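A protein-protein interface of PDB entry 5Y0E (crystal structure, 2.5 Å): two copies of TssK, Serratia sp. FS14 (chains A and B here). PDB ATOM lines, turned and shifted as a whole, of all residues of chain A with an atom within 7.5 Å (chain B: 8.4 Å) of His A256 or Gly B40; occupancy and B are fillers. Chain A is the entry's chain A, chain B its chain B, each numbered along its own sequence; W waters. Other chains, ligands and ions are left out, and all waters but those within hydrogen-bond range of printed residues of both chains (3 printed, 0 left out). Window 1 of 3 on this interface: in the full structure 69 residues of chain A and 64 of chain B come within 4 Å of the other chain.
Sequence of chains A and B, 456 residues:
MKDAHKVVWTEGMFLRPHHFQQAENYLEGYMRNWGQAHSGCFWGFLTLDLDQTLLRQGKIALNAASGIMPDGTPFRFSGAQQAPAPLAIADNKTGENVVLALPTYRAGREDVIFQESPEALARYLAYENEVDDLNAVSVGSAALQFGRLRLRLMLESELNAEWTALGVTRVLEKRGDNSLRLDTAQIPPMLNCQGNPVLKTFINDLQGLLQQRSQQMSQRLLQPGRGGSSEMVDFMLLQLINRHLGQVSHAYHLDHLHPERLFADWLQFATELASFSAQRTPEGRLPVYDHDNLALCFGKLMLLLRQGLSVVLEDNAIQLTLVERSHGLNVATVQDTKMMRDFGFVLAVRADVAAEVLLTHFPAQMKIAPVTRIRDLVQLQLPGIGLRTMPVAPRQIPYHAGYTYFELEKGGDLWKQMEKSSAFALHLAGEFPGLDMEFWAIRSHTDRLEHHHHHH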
ATOM      1  N   LEU A  46      24.076  29.956   7.833  1.00  0.00           N
ATOM      2  CA  LEU A  46      25.312  29.347   8.277  1.00  0.00           C
ATOM      3  C   LEU A  46      26.053  30.242   9.234  1.00  0.00           C
ATOM      4  O   LEU A  46      26.683  29.762  10.166  1.00  0.00           O
ATOM      5  CB  LEU A  46      26.224  29.069   7.093  1.00  0.00           C
ATOM      6  CG  LEU A  46      25.809  27.917   6.231  1.00  0.00           C
ATOM      7  CD1 LEU A  46      26.465  28.111   4.922  1.00  0.00           C
ATOM      8  CD2 LEU A  46      26.272  26.653   6.901  1.00  0.00           C
ATOM      9  N   LEU A 191      21.520  26.750   9.635  1.00  0.00           N
ATOM     10  CA  LEU A 191      21.991  25.567   8.936  1.00  0.00           C
ATOM     11  C   LEU A 191      23.138  24.889   9.649  1.00  0.00           C
ATOM     12  O   LEU A 191      23.374  23.714   9.411  1.00  0.00           O
ATOM     13  CB  LEU A 191      22.409  25.905   7.505  1.00  0.00           C
ATOM     14  CG  LEU A 191      21.181  26.155   6.652  1.00  0.00           C
ATOM     15  CD1 LEU A 191      21.549  26.540   5.261  1.00  0.00           C
ATOM     16  CD2 LEU A 191      20.285  24.957   6.646  1.00  0.00           C
ATOM     17  N   ASN A 192      23.832  25.578  10.534  1.00  0.00           N
ATOM     18  CA  ASN A 192      24.863  24.957  11.336  1.00  0.00           C
ATOM     19  C   ASN A 192      24.664  25.364  12.784  1.00  0.00           C
ATOM     20  O   ASN A 192      24.673  26.550  13.103  1.00  0.00           O
ATOM     21  CB  ASN A 192      26.237  25.369  10.840  1.00  0.00           C
ATOM     22  CG  ASN A 192      27.345  24.676  11.570  1.00  0.00           C
ATOM     23  OD1 ASN A 192      27.131  23.706  12.250  1.00  0.00           O
ATOM     24  ND2 ASN A 192      28.535  25.189  11.438  1.00  0.00           N
ATOM     25  N   CYS A 193      24.518  24.381  13.659  1.00  0.00           N
ATOM     26  CA  CYS A 193      24.427  24.673  15.075  1.00  0.00           C
ATOM     27  C   CYS A 193      25.578  25.536  15.542  1.00  0.00           C
ATOM     28  O   CYS A 193      25.414  26.356  16.445  1.00  0.00           O
ATOM     29  CB  CYS A 193      24.388  23.375  15.885  1.00  0.00           C
ATOM     30  SG  CYS A 193      22.839  22.480  15.794  1.00  0.00           S
ATOM     31  N   GLN A 194      26.741  25.390  14.939  1.00  0.00           N
ATOM     32  CA  GLN A 194      27.875  26.159  15.411  1.00  0.00           C
ATOM     33  C   GLN A 194      27.831  27.613  14.984  1.00  0.00           C
ATOM     34  O   GLN A 194      28.663  28.390  15.438  1.00  0.00           O
ATOM     35  CB  GLN A 194      29.157  25.501  14.942  1.00  0.00           C
ATOM     36  CG  GLN A 194      29.324  24.098  15.479  1.00  0.00           C
ATOM     37  CD  GLN A 194      29.732  24.075  16.936  1.00  0.00           C
ATOM     38  OE1 GLN A 194      30.606  24.819  17.346  1.00  0.00           O
ATOM     39  NE2 GLN A 194      29.107  23.213  17.720  1.00  0.00           N
ATOM     40  N   HIS A 250      30.308  13.947  20.059  1.00  0.00           N
ATOM     41  CA  HIS A 250      30.391  14.111  18.624  1.00  0.00           C
ATOM     42  C   HIS A 250      29.777  15.435  18.198  1.00  0.00           C
ATOM     43  O   HIS A 250      30.365  16.180  17.413  1.00  0.00           O
ATOM     44  CB  HIS A 250      29.700  12.944  17.931  1.00  0.00           C
ATOM     45  CG  HIS A 250      29.971  12.873  16.469  1.00  0.00           C
ATOM     46  ND1 HIS A 250      31.188  12.478  15.959  1.00  0.00           N
ATOM     47  CD2 HIS A 250      29.194  13.168  15.407  1.00  0.00           C
ATOM     48  CE1 HIS A 250      31.138  12.515  14.644  1.00  0.00           C
ATOM     49  NE2 HIS A 250      29.941  12.939  14.284  1.00  0.00           N
ATOM     50  N   ALA A 251      28.589  15.744  18.713  1.00  0.00           N
ATOM     51  CA  ALA A 251      27.949  17.012  18.393  1.00  0.00           C
ATOM     52  C   ALA A 251      28.827  18.181  18.788  1.00  0.00           C
ATOM     53  O   ALA A 251      28.996  19.134  18.028  1.00  0.00           O
ATOM     54  CB  ALA A 251      26.601  17.097  19.098  1.00  0.00           C
ATOM     55  N   HIS A 253      31.990  18.436  19.021  1.00  0.00           N
ATOM     56  CA  HIS A 253      33.208  18.613  18.257  1.00  0.00           C
ATOM     57  C   HIS A 253      32.975  18.818  16.772  1.00  0.00           C
ATOM     58  O   HIS A 253      33.862  19.332  16.098  1.00  0.00           O
ATOM     59  CB  HIS A 253      34.126  17.429  18.482  1.00  0.00           C
ATOM     60  CG  HIS A 253      34.850  17.474  19.784  1.00  0.00           C
ATOM     61  ND1 HIS A 253      34.583  16.605  20.814  1.00  0.00           N
ATOM     62  CD2 HIS A 253      35.833  18.285  20.230  1.00  0.00           C
ATOM     63  CE1 HIS A 253      35.380  16.869  21.832  1.00  0.00           C
ATOM     64  NE2 HIS A 253      36.146  17.888  21.503  1.00  0.00           N
ATOM     65  N   LEU A 254      31.809  18.472  16.252  1.00  0.00           N
ATOM     66  CA  LEU A 254      31.559  18.656  14.836  1.00  0.00           C
ATOM     67  C   LEU A 254      31.669  20.121  14.463  1.00  0.00           C
ATOM     68  O   LEU A 254      31.168  20.995  15.164  1.00  0.00           O
ATOM     69  CB  LEU A 254      30.180  18.145  14.468  1.00  0.00           C
ATOM     70  CG  LEU A 254      29.992  16.669  14.180  1.00  0.00           C
ATOM     71  CD1 LEU A 254      28.553  16.390  13.873  1.00  0.00           C
ATOM     72  CD2 LEU A 254      30.822  16.296  13.019  1.00  0.00           C
ATOM     73  N   ASP A 255      32.362  20.393  13.369  1.00  0.00           N
ATOM     74  CA  ASP A 255      32.411  21.747  12.840  1.00  0.00           C
ATOM     75  C   ASP A 255      31.120  22.143  12.161  1.00  0.00           C
ATOM     76  O   ASP A 255      30.841  23.331  12.032  1.00  0.00           O
ATOM     77  CB  ASP A 255      33.548  21.889  11.834  1.00  0.00           C
ATOM     78  CG  ASP A 255      34.854  22.075  12.491  1.00  0.00           C
ATOM     79  OD1 ASP A 255      34.867  22.322  13.700  1.00  0.00           O
ATOM     80  OD2 ASP A 255      35.870  22.002  11.802  1.00  0.00           O
ATOM     81  N   HIS A 256      30.351  21.180  11.698  1.00  0.00           N
ATOM     82  CA  HIS A 256      29.131  21.469  10.982  1.00  0.00           C
ATOM     83  C   HIS A 256      28.074  20.447  11.362  1.00  0.00           C
ATOM     84  O   HIS A 256      28.305  19.242  11.242  1.00  0.00           O
ATOM     85  CB  HIS A 256      29.393  21.466   9.490  1.00  0.00           C
ATOM     86  CG  HIS A 256      28.187  21.755   8.673  1.00  0.00           C
ATOM     87  ND1 HIS A 256      27.198  20.824   8.459  1.00  0.00           N
ATOM     88  CD2 HIS A 256      27.803  22.870   8.020  1.00  0.00           C
ATOM     89  CE1 HIS A 256      26.259  21.350   7.700  1.00  0.00           C
ATOM     90  NE2 HIS A 256      26.608  22.588   7.411  1.00  0.00           N
ATOM     91  N   LEU A 257      26.926  20.926  11.833  1.00  0.00           N
ATOM     92  CA  LEU A 257      25.853  20.049  12.286  1.00  0.00           C
ATOM     93  C   LEU A 257      24.520  20.762  12.141  1.00  0.00           C
ATOM     94  O   LEU A 257      24.309  21.801  12.765  1.00  0.00           O
ATOM     95  CB  LEU A 257      26.094  19.625  13.725  1.00  0.00           C
ATOM     96  CG  LEU A 257      24.965  18.903  14.435  1.00  0.00           C
ATOM     97  CD1 LEU A 257      24.865  17.492  13.909  1.00  0.00           C
ATOM     98  CD2 LEU A 257      25.211  18.884  15.909  1.00  0.00           C
ATOM     99  N   HIS A 258      23.640  20.211  11.318  1.00  0.00           N
ATOM    100  CA  HIS A 258      22.321  20.785  11.126  1.00  0.00           C
ATOM    101  C   HIS A 258      21.439  20.551  12.359  1.00  0.00           C
ATOM    102  O   HIS A 258      21.438  19.456  12.928  1.00  0.00           O
ATOM    103  CB  HIS A 258      21.670  20.182   9.880  1.00  0.00           C
ATOM    104  CG  HIS A 258      20.381  20.828   9.465  1.00  0.00           C
ATOM    105  ND1 HIS A 258      19.283  20.915  10.288  1.00  0.00           N
ATOM    106  CD2 HIS A 258      20.001  21.369   8.287  1.00  0.00           C
ATOM    107  CE1 HIS A 258      18.290  21.492   9.645  1.00  0.00           C
ATOM    108  NE2 HIS A 258      18.702  21.785   8.430  1.00  0.00           N
ATOM    109  N   PRO A 259      20.681  21.567  12.781  1.00  0.00           N
ATOM    110  CA  PRO A 259      19.834  21.451  13.982  1.00  0.00           C
ATOM    111  C   PRO A 259      18.825  20.328  13.956  1.00  0.00           C
ATOM    112  O   PRO A 259      18.527  19.758  15.002  1.00  0.00           O
ATOM    113  CB  PRO A 259      19.112  22.803  14.014  1.00  0.00           C
ATOM    114  CG  PRO A 259      20.018  23.718  13.317  1.00  0.00           C
ATOM    115  CD  PRO A 259      20.769  22.950  12.299  1.00  0.00           C
ATOM    116  N   ARG A 261      19.125  17.423  12.825  1.00  0.00           N
ATOM    117  CA  ARG A 261      19.747  16.180  13.202  1.00  0.00           C
ATOM    118  C   ARG A 261      19.945  16.124  14.706  1.00  0.00           C
ATOM    119  O   ARG A 261      19.671  15.105  15.345  1.00  0.00           O
ATOM    120  CB  ARG A 261      21.055  16.044  12.431  1.00  0.00           C
ATOM    121  CG  ARG A 261      21.793  14.781  12.656  1.00  0.00           C
ATOM    122  CD  ARG A 261      23.137  14.846  11.996  1.00  0.00           C
ATOM    123  NE  ARG A 261      23.894  13.637  12.248  1.00  0.00           N
ATOM    124  CZ  ARG A 261      25.203  13.553  12.144  1.00  0.00           C
ATOM    125  NH1 ARG A 261      25.891  14.603  11.781  1.00  0.00           N
ATOM    126  NH2 ARG A 261      25.812  12.421  12.415  1.00  0.00           N
ATOM    127  N   TRP B  34      25.806  25.960  -2.222  1.00  0.00           N
ATOM    128  CA  TRP B  34      24.690  25.126  -1.880  1.00  0.00           C
ATOM    129  C   TRP B  34      25.163  23.841  -1.273  1.00  0.00           C
ATOM    130  O   TRP B  34      24.586  23.342  -0.352  1.00  0.00           O
ATOM    131  CB  TRP B  34      23.891  24.795  -3.110  1.00  0.00           C
ATOM    132  CG  TRP B  34      22.519  25.226  -3.051  1.00  0.00           C
ATOM    133  CD1 TRP B  34      22.033  26.355  -3.538  1.00  0.00           C
ATOM    134  CD2 TRP B  34      21.427  24.531  -2.481  1.00  0.00           C
ATOM    135  NE1 TRP B  34      20.707  26.438  -3.313  1.00  0.00           N
ATOM    136  CE2 TRP B  34      20.307  25.320  -2.655  1.00  0.00           C
ATOM    137  CE3 TRP B  34      21.288  23.315  -1.840  1.00  0.00           C
ATOM    138  CZ2 TRP B  34      19.073  24.946  -2.222  1.00  0.00           C
ATOM    139  CZ3 TRP B  34      20.075  22.956  -1.414  1.00  0.00           C
ATOM    140  CH2 TRP B  34      18.979  23.758  -1.605  1.00  0.00           C
ATOM    141  N   GLY B  35      26.236  23.309  -1.803  1.00  0.00           N
ATOM    142  CA  GLY B  35      26.760  22.068  -1.325  1.00  0.00           C
ATOM    143  C   GLY B  35      27.440  22.167  -0.006  1.00  0.00           C
ATOM    144  O   GLY B  35      27.329  21.300   0.805  1.00  0.00           O
ATOM    145  N   GLN B  36      28.159  23.240   0.198  1.00  0.00           N
ATOM    146  CA  GLN B  36      28.869  23.404   1.425  1.00  0.00           C
ATOM    147  C   GLN B  36      27.966  23.784   2.564  1.00  0.00           C
ATOM    148  O   GLN B  36      28.302  23.598   3.697  1.00  0.00           O
ATOM    149  CB  GLN B  36      29.985  24.393   1.243  1.00  0.00           C
ATOM    150  CG  GLN B  36      31.119  23.849   0.423  1.00  0.00           C
ATOM    151  CD  GLN B  36      32.238  24.829   0.283  1.00  0.00           C
ATOM    152  OE1 GLN B  36      32.422  25.682   1.115  1.00  0.00           O
ATOM    153  NE2 GLN B  36      32.984  24.706  -0.763  1.00  0.00           N
ATOM    154  N   ALA B  37      26.805  24.309   2.258  1.00  0.00           N
ATOM    155  CA  ALA B  37      25.867  24.648   3.305  1.00  0.00           C
ATOM    156  C   ALA B  37      25.189  23.425   3.882  1.00  0.00           C
ATOM    157  O   ALA B  37      24.664  23.495   4.986  1.00  0.00           O
ATOM    158  CB  ALA B  37      24.803  25.613   2.789  1.00  0.00           C
ATOM    159  N   HIS B  38      25.192  22.308   3.174  1.00  0.00           N
ATOM    160  CA  HIS B  38      24.494  21.120   3.628  1.00  0.00           C
ATOM    161  C   HIS B  38      25.386  19.898   3.798  1.00  0.00           C
ATOM    162  O   HIS B  38      24.861  18.794   3.935  1.00  0.00           O
ATOM    163  CB  HIS B  38      23.360  20.809   2.670  1.00  0.00           C
ATOM    164  CG  HIS B  38      22.365  21.913   2.567  1.00  0.00           C
ATOM    165  ND1 HIS B  38      22.404  22.858   1.571  1.00  0.00           N
ATOM    166  CD2 HIS B  38      21.327  22.253   3.367  1.00  0.00           C
ATOM    167  CE1 HIS B  38      21.415  23.711   1.739  1.00  0.00           C
ATOM    168  NE2 HIS B  38      20.747  23.367   2.821  1.00  0.00           N
ATOM    169  N   SER B  39      26.706  20.050   3.800  1.00  0.00           N
ATOM    170  CA  SER B  39      27.590  18.917   4.025  1.00  0.00           C
ATOM    171  C   SER B  39      28.806  19.399   4.781  1.00  0.00           C
ATOM    172  O   SER B  39      29.478  20.330   4.343  1.00  0.00           O
ATOM    173  CB  SER B  39      28.021  18.257   2.714  1.00  0.00           C
ATOM    174  OG  SER B  39      26.897  17.816   1.980  1.00  0.00           O
ATOM    175  N   GLY B  40      29.103  18.759   5.889  1.00  0.00           N
ATOM    176  CA  GLY B  40      30.072  19.324   6.778  1.00  0.00           C
ATOM    177  C   GLY B  40      31.467  18.825   6.546  1.00  0.00           C
ATOM    178  O   GLY B  40      32.439  19.504   6.879  1.00  0.00           O
ATOM    179  N   CYS B  41      31.599  17.626   6.023  1.00  0.00           N
ATOM    180  CA  CYS B  41      32.915  17.112   5.677  1.00  0.00           C
ATOM    181  C   CYS B  41      32.892  16.751   4.203  1.00  0.00           C
ATOM    182  O   CYS B  41      32.931  15.581   3.860  1.00  0.00           O
ATOM    183  CB  CYS B  41      33.283  15.942   6.544  1.00  0.00           C
ATOM    184  SG  CYS B  41      33.628  16.382   8.246  1.00  0.00           S
ATOM    185  N   PHE B  42      32.806  17.775   3.355  1.00  0.00           N
ATOM    186  CA  PHE B  42      32.422  17.647   1.961  1.00  0.00           C
ATOM    187  C   PHE B  42      33.565  17.239   1.029  1.00  0.00           C
ATOM    188  O   PHE B  42      33.295  16.952  -0.136  1.00  0.00           O
ATOM    189  CB  PHE B  42      31.828  18.974   1.475  1.00  0.00           C
ATOM    190  CG  PHE B  42      32.773  20.144   1.611  1.00  0.00           C
ATOM    191  CD1 PHE B  42      33.672  20.448   0.611  1.00  0.00           C
ATOM    192  CD2 PHE B  42      32.773  20.924   2.750  1.00  0.00           C
ATOM    193  CE1 PHE B  42      34.541  21.494   0.749  1.00  0.00           C
ATOM    194  CE2 PHE B  42      33.647  21.973   2.882  1.00  0.00           C
ATOM    195  CZ  PHE B  42      34.524  22.258   1.887  1.00  0.00           C
ATOM    196  N   TRP B  43      34.811  17.219   1.497  1.00  0.00           N
ATOM    197  CA  TRP B  43      35.973  16.942   0.666  1.00  0.00           C
ATOM    198  C   TRP B  43      36.543  15.556   0.927  1.00  0.00           C
ATOM    199  O   TRP B  43      36.471  15.031   2.037  1.00  0.00           O
ATOM    200  CB  TRP B  43      37.082  17.959   0.908  1.00  0.00           C
ATOM    201  CG  TRP B  43      37.622  17.907   2.279  1.00  0.00           C
ATOM    202  CD1 TRP B  43      38.739  17.270   2.694  1.00  0.00           C
ATOM    203  CD2 TRP B  43      37.060  18.525   3.430  1.00  0.00           C
ATOM    204  NE1 TRP B  43      38.920  17.449   4.042  1.00  0.00           N
ATOM    205  CE2 TRP B  43      37.902  18.226   4.516  1.00  0.00           C
ATOM    206  CE3 TRP B  43      35.928  19.313   3.651  1.00  0.00           C
ATOM    207  CZ2 TRP B  43      37.641  18.674   5.800  1.00  0.00           C
ATOM    208  CZ3 TRP B  43      35.676  19.755   4.916  1.00  0.00           C
ATOM    209  CH2 TRP B  43      36.523  19.434   5.979  1.00  0.00           C
ATOM    210  N   LEU B 191      34.911  10.210   1.158  1.00  0.00           N
ATOM    211  CA  LEU B 191      33.514  10.540   1.129  1.00  0.00           C
ATOM    212  C   LEU B 191      32.652   9.301   1.152  1.00  0.00           C
ATOM    213  O   LEU B 191      31.439   9.407   1.288  1.00  0.00           O
ATOM    214  CB  LEU B 191      33.214  11.378  -0.108  1.00  0.00           C
ATOM    215  CG  LEU B 191      33.820  12.785  -0.135  1.00  0.00           C
ATOM    216  CD1 LEU B 191      33.268  13.578  -1.318  1.00  0.00           C
ATOM    217  CD2 LEU B 191      33.569  13.529   1.176  1.00  0.00           C
ATOM    218  N   HIS B 258      28.999   7.921   4.270  1.00  0.00           N
ATOM    219  CA  HIS B 258      30.048   8.827   4.685  1.00  0.00           C
ATOM    220  C   HIS B 258      30.652   8.360   6.004  1.00  0.00           C
ATOM    221  O   HIS B 258      29.941   7.923   6.897  1.00  0.00           O
ATOM    222  CB  HIS B 258      29.502  10.240   4.819  1.00  0.00           C
ATOM    223  CG  HIS B 258      30.557  11.293   4.950  1.00  0.00           C
ATOM    224  ND1 HIS B 258      31.454  11.327   5.993  1.00  0.00           N
ATOM    225  CD2 HIS B 258      30.824  12.378   4.192  1.00  0.00           C
ATOM    226  CE1 HIS B 258      32.233  12.380   5.865  1.00  0.00           C
ATOM    227  NE2 HIS B 258      31.864  13.039   4.786  1.00  0.00           N
ATOM    228  N   GLU B 260      31.758   9.958   8.539  1.00  0.00           N
ATOM    229  CA  GLU B 260      31.340  10.696   9.724  1.00  0.00           C
ATOM    230  C   GLU B 260      30.082  10.084  10.311  1.00  0.00           C
ATOM    231  O   GLU B 260      29.966   9.920  11.524  1.00  0.00           O
ATOM    232  CB  GLU B 260      31.119  12.162   9.365  1.00  0.00           C
ATOM    233  CG  GLU B 260      30.651  13.082  10.487  1.00  0.00           C
ATOM    234  CD  GLU B 260      29.140  13.076  10.715  1.00  0.00           C
ATOM    235  OE1 GLU B 260      28.360  12.967   9.759  1.00  0.00           O
ATOM    236  OE2 GLU B 260      28.746  13.132  11.875  1.00  0.00           O
ATOM    237  N   TYR B 289      36.191  12.819  15.857  1.00  0.00           N
ATOM    238  CA  TYR B 289      36.271  12.590  14.425  1.00  0.00           C
ATOM    239  C   TYR B 289      37.227  13.578  13.781  1.00  0.00           C
ATOM    240  O   TYR B 289      37.144  14.786  14.012  1.00  0.00           O
ATOM    241  CB  TYR B 289      34.904  12.720  13.798  1.00  0.00           C
ATOM    242  CG  TYR B 289      34.876  12.438  12.330  1.00  0.00           C
ATOM    243  CD1 TYR B 289      34.909  11.142  11.858  1.00  0.00           C
ATOM    244  CD2 TYR B 289      34.795  13.457  11.411  1.00  0.00           C
ATOM    245  CE1 TYR B 289      34.860  10.878  10.525  1.00  0.00           C
ATOM    246  CE2 TYR B 289      34.744  13.193  10.077  1.00  0.00           C
ATOM    247  CZ  TYR B 289      34.781  11.904   9.641  1.00  0.00           C
ATOM    248  OH  TYR B 289      34.732  11.622   8.308  1.00  0.00           O
ATOM    249  N   HIS B 291      38.394  14.150   9.916  1.00  0.00           N
ATOM    250  CA  HIS B 291      38.180  13.703   8.557  1.00  0.00           C
ATOM    251  C   HIS B 291      39.478  13.533   7.788  1.00  0.00           C
ATOM    252  O   HIS B 291      39.503  12.812   6.789  1.00  0.00           O
ATOM    253  CB  HIS B 291      37.291  14.701   7.856  1.00  0.00           C
ATOM    254  CG  HIS B 291      36.741  14.211   6.568  1.00  0.00           C
ATOM    255  ND1 HIS B 291      35.830  13.187   6.497  1.00  0.00           N
ATOM    256  CD2 HIS B 291      36.955  14.618   5.299  1.00  0.00           C
ATOM    257  CE1 HIS B 291      35.505  12.979   5.236  1.00  0.00           C
ATOM    258  NE2 HIS B 291      36.180  13.831   4.490  1.00  0.00           N
HETATM  259  O   HOH W   1      33.372  13.080  17.026  1.00  0.00           O
HETATM  260  O   HOH W   2      32.071  18.675  10.695  1.00  0.00           O
HETATM  261  O   HOH W   3      25.728  12.338   9.348  1.00  0.00           O
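NE2 of His A250 sits at hydrogen-bond distance from OE2 of Glu B260 (2.7 Å).
A ring nitrogen (NE2) of His A256 sits at hydrogen-bond distance from the backbone carbonyl oxygen (O) of Ala B37.
The guanidinium group (NH2) of Arg A261 is in salt-bridge range of the side-chain carboxylate (OE2) of Glu B260 (3.1 Å).
A ring nitrogen (ND1) of His B258 lies within hydrogen-bond range of the backbone NH (N) of Glu B260, 2.9 Å away.
N of Glu B260 sits at hydrogen-bond distance from OH of Tyr B289 (3.4 Å).
OH of Tyr B289 lies within hydrogen-bond range of ND1 of His B291.
Hydrophobic or aromatic side chains of chain B within 4 Å of the printed part of chain A: Ala B37 and Tyr B289.
Of the 15 printed residues of chain A, 5 touch a printed residue of chain B.
Printed residues of chain A that touch a printed residue of chain B: Leu A46, His A250, Leu A254, His A256 and Arg A261.
Hydrophobic or aromatic side chains of chain A within 4 Å of the printed part of chain B: Leu A46, His A250, Leu A254 and His A256.
Along chain A the printed residues that touch a printed residue of chain B span positions 46 to 261.
Among the printed residues, Asp or Glu carboxylates within 4 Å of a Lys or Arg side-chain nitrogen of the other chain: Arg A261 with Glu B260 (3.1 Å).
Water W1 lies within hydrogen-bond range of ND1 of His A250 (2.5 Å) and N of Tyr B289 (3.1 Å).
Water W3 lies within hydrogen-bond range of OE1 of Glu B260 (2.7 Å) and NH2 of Arg A261 (3.1 Å).
Water W2 lies within hydrogen-bond range of the backbone NH (N) of Asp A255 (3.2 Å), the backbone NH (N) of His A256 (3.2 Å) and the side-chain sulfur (SG) of Cys B41 (3.7 Å).
Of the printed residues of chain B, Leu A254 touches Glu B260.
His A256 touches just these residues of chain B: Ala B37 (3.2 Å) and Gly B40 (3.5 Å).
Gly B40 touches just one residue of chain A: His A256 (3.5 Å).
Printed residues of chain A within 4 Å of Tyr B289: His A250.
His B291 touches none of the printed residues of chain A.
Ala B37 touches Leu A46 (CB to CD1, 3.7 Å).
Tyr B289 touches His A250.
Glu B260 touches Leu A254 (OE2 to CD1, 3.8 Å).
CB of His A256 touches CA of Gly B40, 3.5 Å away.
Positions printed for both chains: 191 and 258.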
